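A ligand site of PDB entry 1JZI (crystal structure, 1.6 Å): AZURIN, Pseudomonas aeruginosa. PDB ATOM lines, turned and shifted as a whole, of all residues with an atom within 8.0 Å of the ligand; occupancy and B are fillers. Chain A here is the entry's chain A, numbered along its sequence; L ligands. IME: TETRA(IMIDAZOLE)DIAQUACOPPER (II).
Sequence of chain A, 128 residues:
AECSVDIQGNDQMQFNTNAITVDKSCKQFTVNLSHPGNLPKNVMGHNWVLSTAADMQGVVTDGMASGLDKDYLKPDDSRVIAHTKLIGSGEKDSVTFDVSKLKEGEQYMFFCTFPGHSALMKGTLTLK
A nitrogen (NDB) of the ligand lies within hydrogen-bond range of the side-chain amino group (NZ) of Lys 27, at 3.1 Å.
ND5 of the ligand lies close to N of Ser 100 (3.5 Å).
O of Lys 128 is in salt-bridge range of NZ of Lys 24 (3.1 Å).
O of Lys 27 lies within hydrogen-bond range of N of Val 99 (3.0 Å).
An oxygen (O1) of the ligand sits close to the backbone carbonyl oxygen of Lys 24 (2.8 Å).
O of Cys 26 sits close to O1 of the ligand, 2.9 Å away.
The backbone carbonyl oxygen (O) of Leu 102 lies close to a nitrogen (NDV) of the ligand (2.8 Å).
Residues that only touch the ligand: Val 99 (3.6 Å) and Leu 127 (3.7 Å).
Hydrophobic or aromatic side chains that line the ligand: Val 99 and Leu 127.
Within 4 Å of the ligand: Lys 24, Cys 26, Lys 27, Val 99, Ser 100, Leu 102 and Leu 127.
The nearest printed residue that does not touch the ligand is Ser 25 (4.2 Å).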
ATOM      1  N   VAL A  22     -26.799   1.882 -24.049  1.00  0.00           N
ATOM      2  CA  VAL A  22     -26.371   1.565 -22.694  1.00  0.00           C
ATOM      3  C   VAL A  22     -24.867   1.320 -22.722  1.00  0.00           C
ATOM      4  O   VAL A  22     -24.385   0.458 -23.458  1.00  0.00           O
ATOM      5  CB  VAL A  22     -27.105   0.316 -22.138  1.00  0.00           C
ATOM      6  CG1 VAL A  22     -26.637   0.005 -20.717  1.00  0.00           C
ATOM      7  CG2 VAL A  22     -28.613   0.546 -22.148  1.00  0.00           C
ATOM      8  N   ASP A  23     -24.131   2.124 -21.956  1.00  0.00           N
ATOM      9  CA  ASP A  23     -22.676   2.007 -21.879  1.00  0.00           C
ATOM     10  C   ASP A  23     -22.293   0.748 -21.109  1.00  0.00           C
ATOM     11  O   ASP A  23     -22.879   0.457 -20.063  1.00  0.00           O
ATOM     12  CB  ASP A  23     -22.101   3.252 -21.191  1.00  0.00           C
ATOM     13  CG  ASP A  23     -20.601   3.372 -21.361  1.00  0.00           C
ATOM     14  OD1 ASP A  23     -19.857   2.526 -20.824  1.00  0.00           O
ATOM     15  OD2 ASP A  23     -20.160   4.328 -22.044  1.00  0.00           O
ATOM     16  N   LYS A  24     -21.316   0.005 -21.624  1.00  0.00           N
ATOM     17  CA  LYS A  24     -20.845  -1.226 -20.997  1.00  0.00           C
ATOM     18  C   LYS A  24     -20.339  -1.048 -19.579  1.00  0.00           C
ATOM     19  O   LYS A  24     -20.418  -1.979 -18.772  1.00  0.00           O
ATOM     20  CB  LYS A  24     -19.718  -1.862 -21.814  1.00  0.00           C
ATOM     21  CG  LYS A  24     -20.124  -2.373 -23.160  1.00  0.00           C
ATOM     22  CD  LYS A  24     -19.157  -3.451 -23.627  1.00  0.00           C
ATOM     23  CE  LYS A  24     -17.709  -2.982 -23.648  1.00  0.00           C
ATOM     24  NZ  LYS A  24     -17.448  -1.922 -24.665  1.00  0.00           N
ATOM     25  N   SER A  25     -19.769   0.116 -19.299  1.00  0.00           N
ATOM     26  CA  SER A  25     -19.231   0.416 -17.972  1.00  0.00           C
ATOM     27  C   SER A  25     -20.320   0.376 -16.924  1.00  0.00           C
ATOM     28  O   SER A  25     -20.045   0.268 -15.730  1.00  0.00           O
ATOM     29  CB  SER A  25     -18.571   1.795 -17.968  1.00  0.00           C
ATOM     30  OG  SER A  25     -17.521   1.849 -18.921  1.00  0.00           O
ATOM     31  N   CYS A  26     -21.581   0.459 -17.374  1.00  0.00           N
ATOM     32  CA  CYS A  26     -22.718   0.428 -16.471  1.00  0.00           C
ATOM     33  C   CYS A  26     -23.065  -0.989 -16.026  1.00  0.00           C
ATOM     34  O   CYS A  26     -23.233  -1.875 -16.862  1.00  0.00           O
ATOM     35  CB  CYS A  26     -23.962   1.021 -17.141  1.00  0.00           C
ATOM     36  SG  CYS A  26     -23.825   2.771 -17.610  1.00  0.00           S
ATOM     37  N   LYS A  27     -23.153  -1.193 -14.718  1.00  0.00           N
ATOM     38  CA  LYS A  27     -23.531  -2.495 -14.194  1.00  0.00           C
ATOM     39  C   LYS A  27     -25.072  -2.550 -14.152  1.00  0.00           C
ATOM     40  O   LYS A  27     -25.683  -3.606 -14.258  1.00  0.00           O
ATOM     41  CB  LYS A  27     -22.951  -2.690 -12.789  1.00  0.00           C
ATOM     42  CG  LYS A  27     -21.574  -3.327 -12.748  1.00  0.00           C
ATOM     43  CD  LYS A  27     -21.219  -3.702 -11.325  1.00  0.00           C
ATOM     44  CE  LYS A  27     -20.070  -4.701 -11.256  1.00  0.00           C
ATOM     45  NZ  LYS A  27     -18.862  -4.255 -12.013  1.00  0.00           N
ATOM     46  N   GLN A  28     -25.675  -1.374 -13.998  1.00  0.00           N
ATOM     47  CA  GLN A  28     -27.134  -1.227 -13.948  1.00  0.00           C
ATOM     48  C   GLN A  28     -27.535   0.000 -14.753  1.00  0.00           C
ATOM     49  O   GLN A  28     -26.723   0.911 -14.946  1.00  0.00           O
ATOM     50  CB  GLN A  28     -27.603  -1.065 -12.497  1.00  0.00           C
ATOM     51  CG  GLN A  28     -27.230  -2.254 -11.644  1.00  0.00           C
ATOM     52  CD  GLN A  28     -28.046  -2.338 -10.381  1.00  0.00           C
ATOM     53  OE1 GLN A  28     -28.130  -1.385  -9.617  1.00  0.00           O
ATOM     54  NE2 GLN A  28     -28.670  -3.490 -10.170  1.00  0.00           N
ATOM     55  N   PHE A  29     -28.780   0.024 -15.227  1.00  0.00           N
ATOM     56  CA  PHE A  29     -29.272   1.139 -16.034  1.00  0.00           C
ATOM     57  C   PHE A  29     -30.653   1.541 -15.531  1.00  0.00           C
ATOM     58  O   PHE A  29     -31.481   0.686 -15.219  1.00  0.00           O
ATOM     59  CB  PHE A  29     -29.349   0.727 -17.509  1.00  0.00           C
ATOM     60  CG  PHE A  29     -29.429   1.881 -18.461  1.00  0.00           C
ATOM     61  CD1 PHE A  29     -28.310   2.678 -18.698  1.00  0.00           C
ATOM     62  CD2 PHE A  29     -30.616   2.210 -19.104  1.00  0.00           C
ATOM     63  CE1 PHE A  29     -28.372   3.768 -19.557  1.00  0.00           C
ATOM     64  CE2 PHE A  29     -30.686   3.293 -19.973  1.00  0.00           C
ATOM     65  CZ  PHE A  29     -29.560   4.075 -20.194  1.00  0.00           C
ATOM     66  N   PHE A  97     -32.577  -1.785 -13.991  1.00  0.00           N
ATOM     67  CA  PHE A  97     -32.346  -3.201 -14.275  1.00  0.00           C
ATOM     68  C   PHE A  97     -30.865  -3.514 -14.475  1.00  0.00           C
ATOM     69  O   PHE A  97     -30.060  -2.611 -14.719  1.00  0.00           O
ATOM     70  CB  PHE A  97     -33.168  -3.650 -15.514  1.00  0.00           C
ATOM     71  CG  PHE A  97     -32.775  -2.963 -16.799  1.00  0.00           C
ATOM     72  CD1 PHE A  97     -33.279  -1.712 -17.112  1.00  0.00           C
ATOM     73  CD2 PHE A  97     -31.882  -3.570 -17.686  1.00  0.00           C
ATOM     74  CE1 PHE A  97     -32.906  -1.055 -18.287  1.00  0.00           C
ATOM     75  CE2 PHE A  97     -31.503  -2.925 -18.867  1.00  0.00           C
ATOM     76  CZ  PHE A  97     -32.013  -1.660 -19.164  1.00  0.00           C
ATOM     77  N   ASP A  98     -30.511  -4.798 -14.329  1.00  0.00           N
ATOM     78  CA  ASP A  98     -29.122  -5.245 -14.494  1.00  0.00           C
ATOM     79  C   ASP A  98     -28.734  -5.256 -15.966  1.00  0.00           C
ATOM     80  O   ASP A  98     -29.376  -5.907 -16.782  1.00  0.00           O
ATOM     81  CB  ASP A  98     -28.954  -6.654 -13.911  1.00  0.00           C
ATOM     82  CG  ASP A  98     -28.702  -6.642 -12.429  1.00  0.00           C
ATOM     83  OD1 ASP A  98     -29.581  -6.185 -11.666  1.00  0.00           O
ATOM     84  OD2 ASP A  98     -27.612  -7.093 -12.016  1.00  0.00           O
ATOM     85  N   VAL A  99     -27.651  -4.547 -16.277  1.00  0.00           N
ATOM     86  CA  VAL A  99     -27.175  -4.464 -17.658  1.00  0.00           C
ATOM     87  C   VAL A  99     -26.666  -5.814 -18.164  1.00  0.00           C
ATOM     88  O   VAL A  99     -26.604  -6.051 -19.376  1.00  0.00           O
ATOM     89  CB  VAL A  99     -26.084  -3.370 -17.792  1.00  0.00           C
ATOM     90  CG1 VAL A  99     -25.506  -3.364 -19.201  1.00  0.00           C
ATOM     91  CG2 VAL A  99     -26.693  -1.995 -17.484  1.00  0.00           C
ATOM     92  N   SER A 100     -26.400  -6.727 -17.232  1.00  0.00           N
ATOM     93  CA  SER A 100     -25.924  -8.054 -17.592  1.00  0.00           C
ATOM     94  C   SER A 100     -26.989  -8.837 -18.354  1.00  0.00           C
ATOM     95  O   SER A 100     -26.712  -9.902 -18.895  1.00  0.00           O
ATOM     96  CB  SER A 100     -25.491  -8.830 -16.341  1.00  0.00           C
ATOM     97  OG  SER A 100     -26.572  -8.984 -15.439  1.00  0.00           O
ATOM     98  N   LYS A 101     -28.214  -8.315 -18.366  1.00  0.00           N
ATOM     99  CA  LYS A 101     -29.311  -8.960 -19.086  1.00  0.00           C
ATOM    100  C   LYS A 101     -29.236  -8.631 -20.587  1.00  0.00           C
ATOM    101  O   LYS A 101     -30.028  -9.126 -21.382  1.00  0.00           O
ATOM    102  CB  LYS A 101     -30.657  -8.491 -18.535  1.00  0.00           C
ATOM    103  CG  LYS A 101     -30.801  -8.695 -17.046  1.00  0.00           C
ATOM    104  CD  LYS A 101     -32.127  -8.151 -16.544  1.00  0.00           C
ATOM    105  CE  LYS A 101     -32.156  -8.128 -15.018  1.00  0.00           C
ATOM    106  NZ  LYS A 101     -31.856  -9.465 -14.437  1.00  0.00           N
ATOM    107  N   LEU A 102     -28.289  -7.771 -20.947  1.00  0.00           N
ATOM    108  CA  LEU A 102     -28.089  -7.356 -22.330  1.00  0.00           C
ATOM    109  C   LEU A 102     -26.724  -7.819 -22.818  1.00  0.00           C
ATOM    110  O   LEU A 102     -25.796  -7.973 -22.016  1.00  0.00           O
ATOM    111  CB  LEU A 102     -28.149  -5.828 -22.430  1.00  0.00           C
ATOM    112  CG  LEU A 102     -29.309  -5.072 -21.796  1.00  0.00           C
ATOM    113  CD1 LEU A 102     -29.100  -3.577 -21.988  1.00  0.00           C
ATOM    114  CD2 LEU A 102     -30.641  -5.499 -22.399  1.00  0.00           C
ATOM    115  N   LYS A 103     -26.614  -8.041 -24.122  1.00  0.00           N
ATOM    116  CA  LYS A 103     -25.360  -8.454 -24.722  1.00  0.00           C
ATOM    117  C   LYS A 103     -25.061  -7.638 -25.970  1.00  0.00           C
ATOM    118  O   LYS A 103     -25.975  -7.160 -26.649  1.00  0.00           O
ATOM    119  CB  LYS A 103     -25.363  -9.960 -25.054  1.00  0.00           C
ATOM    120  CG  LYS A 103     -26.295 -10.387 -26.178  1.00  0.00           C
ATOM    121  CD  LYS A 103     -26.230 -11.900 -26.384  1.00  0.00           C
ATOM    122  CE  LYS A 103     -27.063 -12.349 -27.573  1.00  0.00           C
ATOM    123  NZ  LYS A 103     -27.078 -13.830 -27.746  1.00  0.00           N
ATOM    124  N   GLU A 104     -23.775  -7.412 -26.218  1.00  0.00           N
ATOM    125  CA  GLU A 104     -23.344  -6.666 -27.377  1.00  0.00           C
ATOM    126  C   GLU A 104     -23.733  -7.359 -28.671  1.00  0.00           C
ATOM    127  O   GLU A 104     -23.823  -8.585 -28.736  1.00  0.00           O
ATOM    128  CB  GLU A 104     -21.827  -6.490 -27.372  1.00  0.00           C
ATOM    129  CG  GLU A 104     -21.342  -5.169 -26.811  1.00  0.00           C
ATOM    130  CD  GLU A 104     -19.862  -4.957 -27.060  1.00  0.00           C
ATOM    131  OE1 GLU A 104     -19.061  -5.313 -26.168  1.00  0.00           O
ATOM    132  OE2 GLU A 104     -19.512  -4.440 -28.137  1.00  0.00           O
ATOM    133  N   TYR A 108     -32.153  -4.544 -29.482  1.00  0.00           N
ATOM    134  CA  TYR A 108     -33.220  -4.467 -28.494  1.00  0.00           C
ATOM    135  C   TYR A 108     -34.157  -3.325 -28.876  1.00  0.00           C
ATOM    136  O   TYR A 108     -33.787  -2.431 -29.646  1.00  0.00           O
ATOM    137  CB  TYR A 108     -32.661  -4.212 -27.090  1.00  0.00           C
ATOM    138  CG  TYR A 108     -31.711  -5.288 -26.598  1.00  0.00           C
ATOM    139  CD1 TYR A 108     -32.192  -6.488 -26.074  1.00  0.00           C
ATOM    140  CD2 TYR A 108     -30.334  -5.116 -26.683  1.00  0.00           C
ATOM    141  CE1 TYR A 108     -31.329  -7.492 -25.655  1.00  0.00           C
ATOM    142  CE2 TYR A 108     -29.453  -6.114 -26.274  1.00  0.00           C
ATOM    143  CZ  TYR A 108     -29.955  -7.292 -25.759  1.00  0.00           C
ATOM    144  OH  TYR A 108     -29.087  -8.285 -25.384  1.00  0.00           O
ATOM    145  N   LEU A 127     -26.289  -2.292 -26.429  1.00  0.00           N
ATOM    146  CA  LEU A 127     -25.238  -2.287 -25.424  1.00  0.00           C
ATOM    147  C   LEU A 127     -23.951  -2.009 -26.208  1.00  0.00           C
ATOM    148  O   LEU A 127     -23.648  -2.721 -27.176  1.00  0.00           O
ATOM    149  CB  LEU A 127     -25.151  -3.643 -24.709  1.00  0.00           C
ATOM    150  CG  LEU A 127     -24.076  -3.783 -23.620  1.00  0.00           C
ATOM    151  CD1 LEU A 127     -24.287  -2.749 -22.540  1.00  0.00           C
ATOM    152  CD2 LEU A 127     -24.126  -5.175 -23.028  1.00  0.00           C
ATOM    153  N   LYS A 128     -23.242  -0.954 -25.827  1.00  0.00           N
ATOM    154  CA  LYS A 128     -22.021  -0.560 -26.516  1.00  0.00           C
ATOM    155  C   LYS A 128     -20.963   0.047 -25.580  1.00  0.00           C
ATOM    156  O   LYS A 128     -19.769  -0.217 -25.821  1.00  0.00           O
ATOM    157  CB  LYS A 128     -22.373   0.421 -27.644  1.00  0.00           C
ATOM    158  CG  LYS A 128     -21.195   1.003 -28.400  1.00  0.00           C
ATOM    159  CD  LYS A 128     -21.637   1.588 -29.725  1.00  0.00           C
ATOM    160  CE  LYS A 128     -22.833   2.521 -29.583  1.00  0.00           C
ATOM    161  NZ  LYS A 128     -23.295   3.054 -30.897  1.00  0.00           N
ATOM    162  OXT LYS A 128     -21.344   0.762 -24.634  1.00  0.00           O
HETATM  163 CU   IME L   1     -20.787  -6.152 -17.548  1.00  0.00          CU
HETATM  164  O1  IME L   1     -22.107  -4.114 -18.267  1.00  0.00           O
HETATM  165  O2  IME L   1     -19.634  -8.348 -17.101  1.00  0.00           O
HETATM  166  CG1 IME L   1     -18.426  -3.593 -15.228  1.00  0.00           C
HETATM  167  CDC IME L   1     -19.442  -3.844 -16.087  1.00  0.00           C
HETATM  168  NDB IME L   1     -17.880  -4.795 -14.860  1.00  0.00           N
HETATM  169  CEB IME L   1     -18.567  -5.730 -15.500  1.00  0.00           C
HETATM  170  NEC IME L   1     -19.533  -5.210 -16.260  1.00  0.00           N
HETATM  171  CG2 IME L   1     -17.680  -6.516 -20.404  1.00  0.00           C
HETATM  172  CDM IME L   1     -18.709  -6.990 -19.668  1.00  0.00           C
HETATM  173  NDL IME L   1     -17.595  -5.162 -20.155  1.00  0.00           N
HETATM  174  CEL IME L   1     -18.593  -4.993 -19.298  1.00  0.00           C
HETATM  175  NEM IME L   1     -19.341  -6.020 -18.919  1.00  0.00           N
HETATM  176  CG3 IME L   1     -22.977  -8.791 -19.824  1.00  0.00           C
HETATM  177  CDW IME L   1     -22.049  -8.496 -18.883  1.00  0.00           C
HETATM  178  NDV IME L   1     -23.512  -7.638 -20.354  1.00  0.00           N
HETATM  179  CEV IME L   1     -22.859  -6.702 -19.698  1.00  0.00           C
HETATM  180  NEW IME L   1     -21.981  -7.127 -18.808  1.00  0.00           N
HETATM  181  CG4 IME L   1     -23.082  -6.591 -13.875  1.00  0.00           C
HETATM  182  CD6 IME L   1     -21.939  -6.647 -14.598  1.00  0.00           C
HETATM  183  ND5 IME L   1     -23.943  -6.152 -14.850  1.00  0.00           N
HETATM  184  CE5 IME L   1     -23.177  -6.035 -15.910  1.00  0.00           C
HETATM  185  NE6 IME L   1     -21.882  -6.304 -15.927  1.00  0.00           N
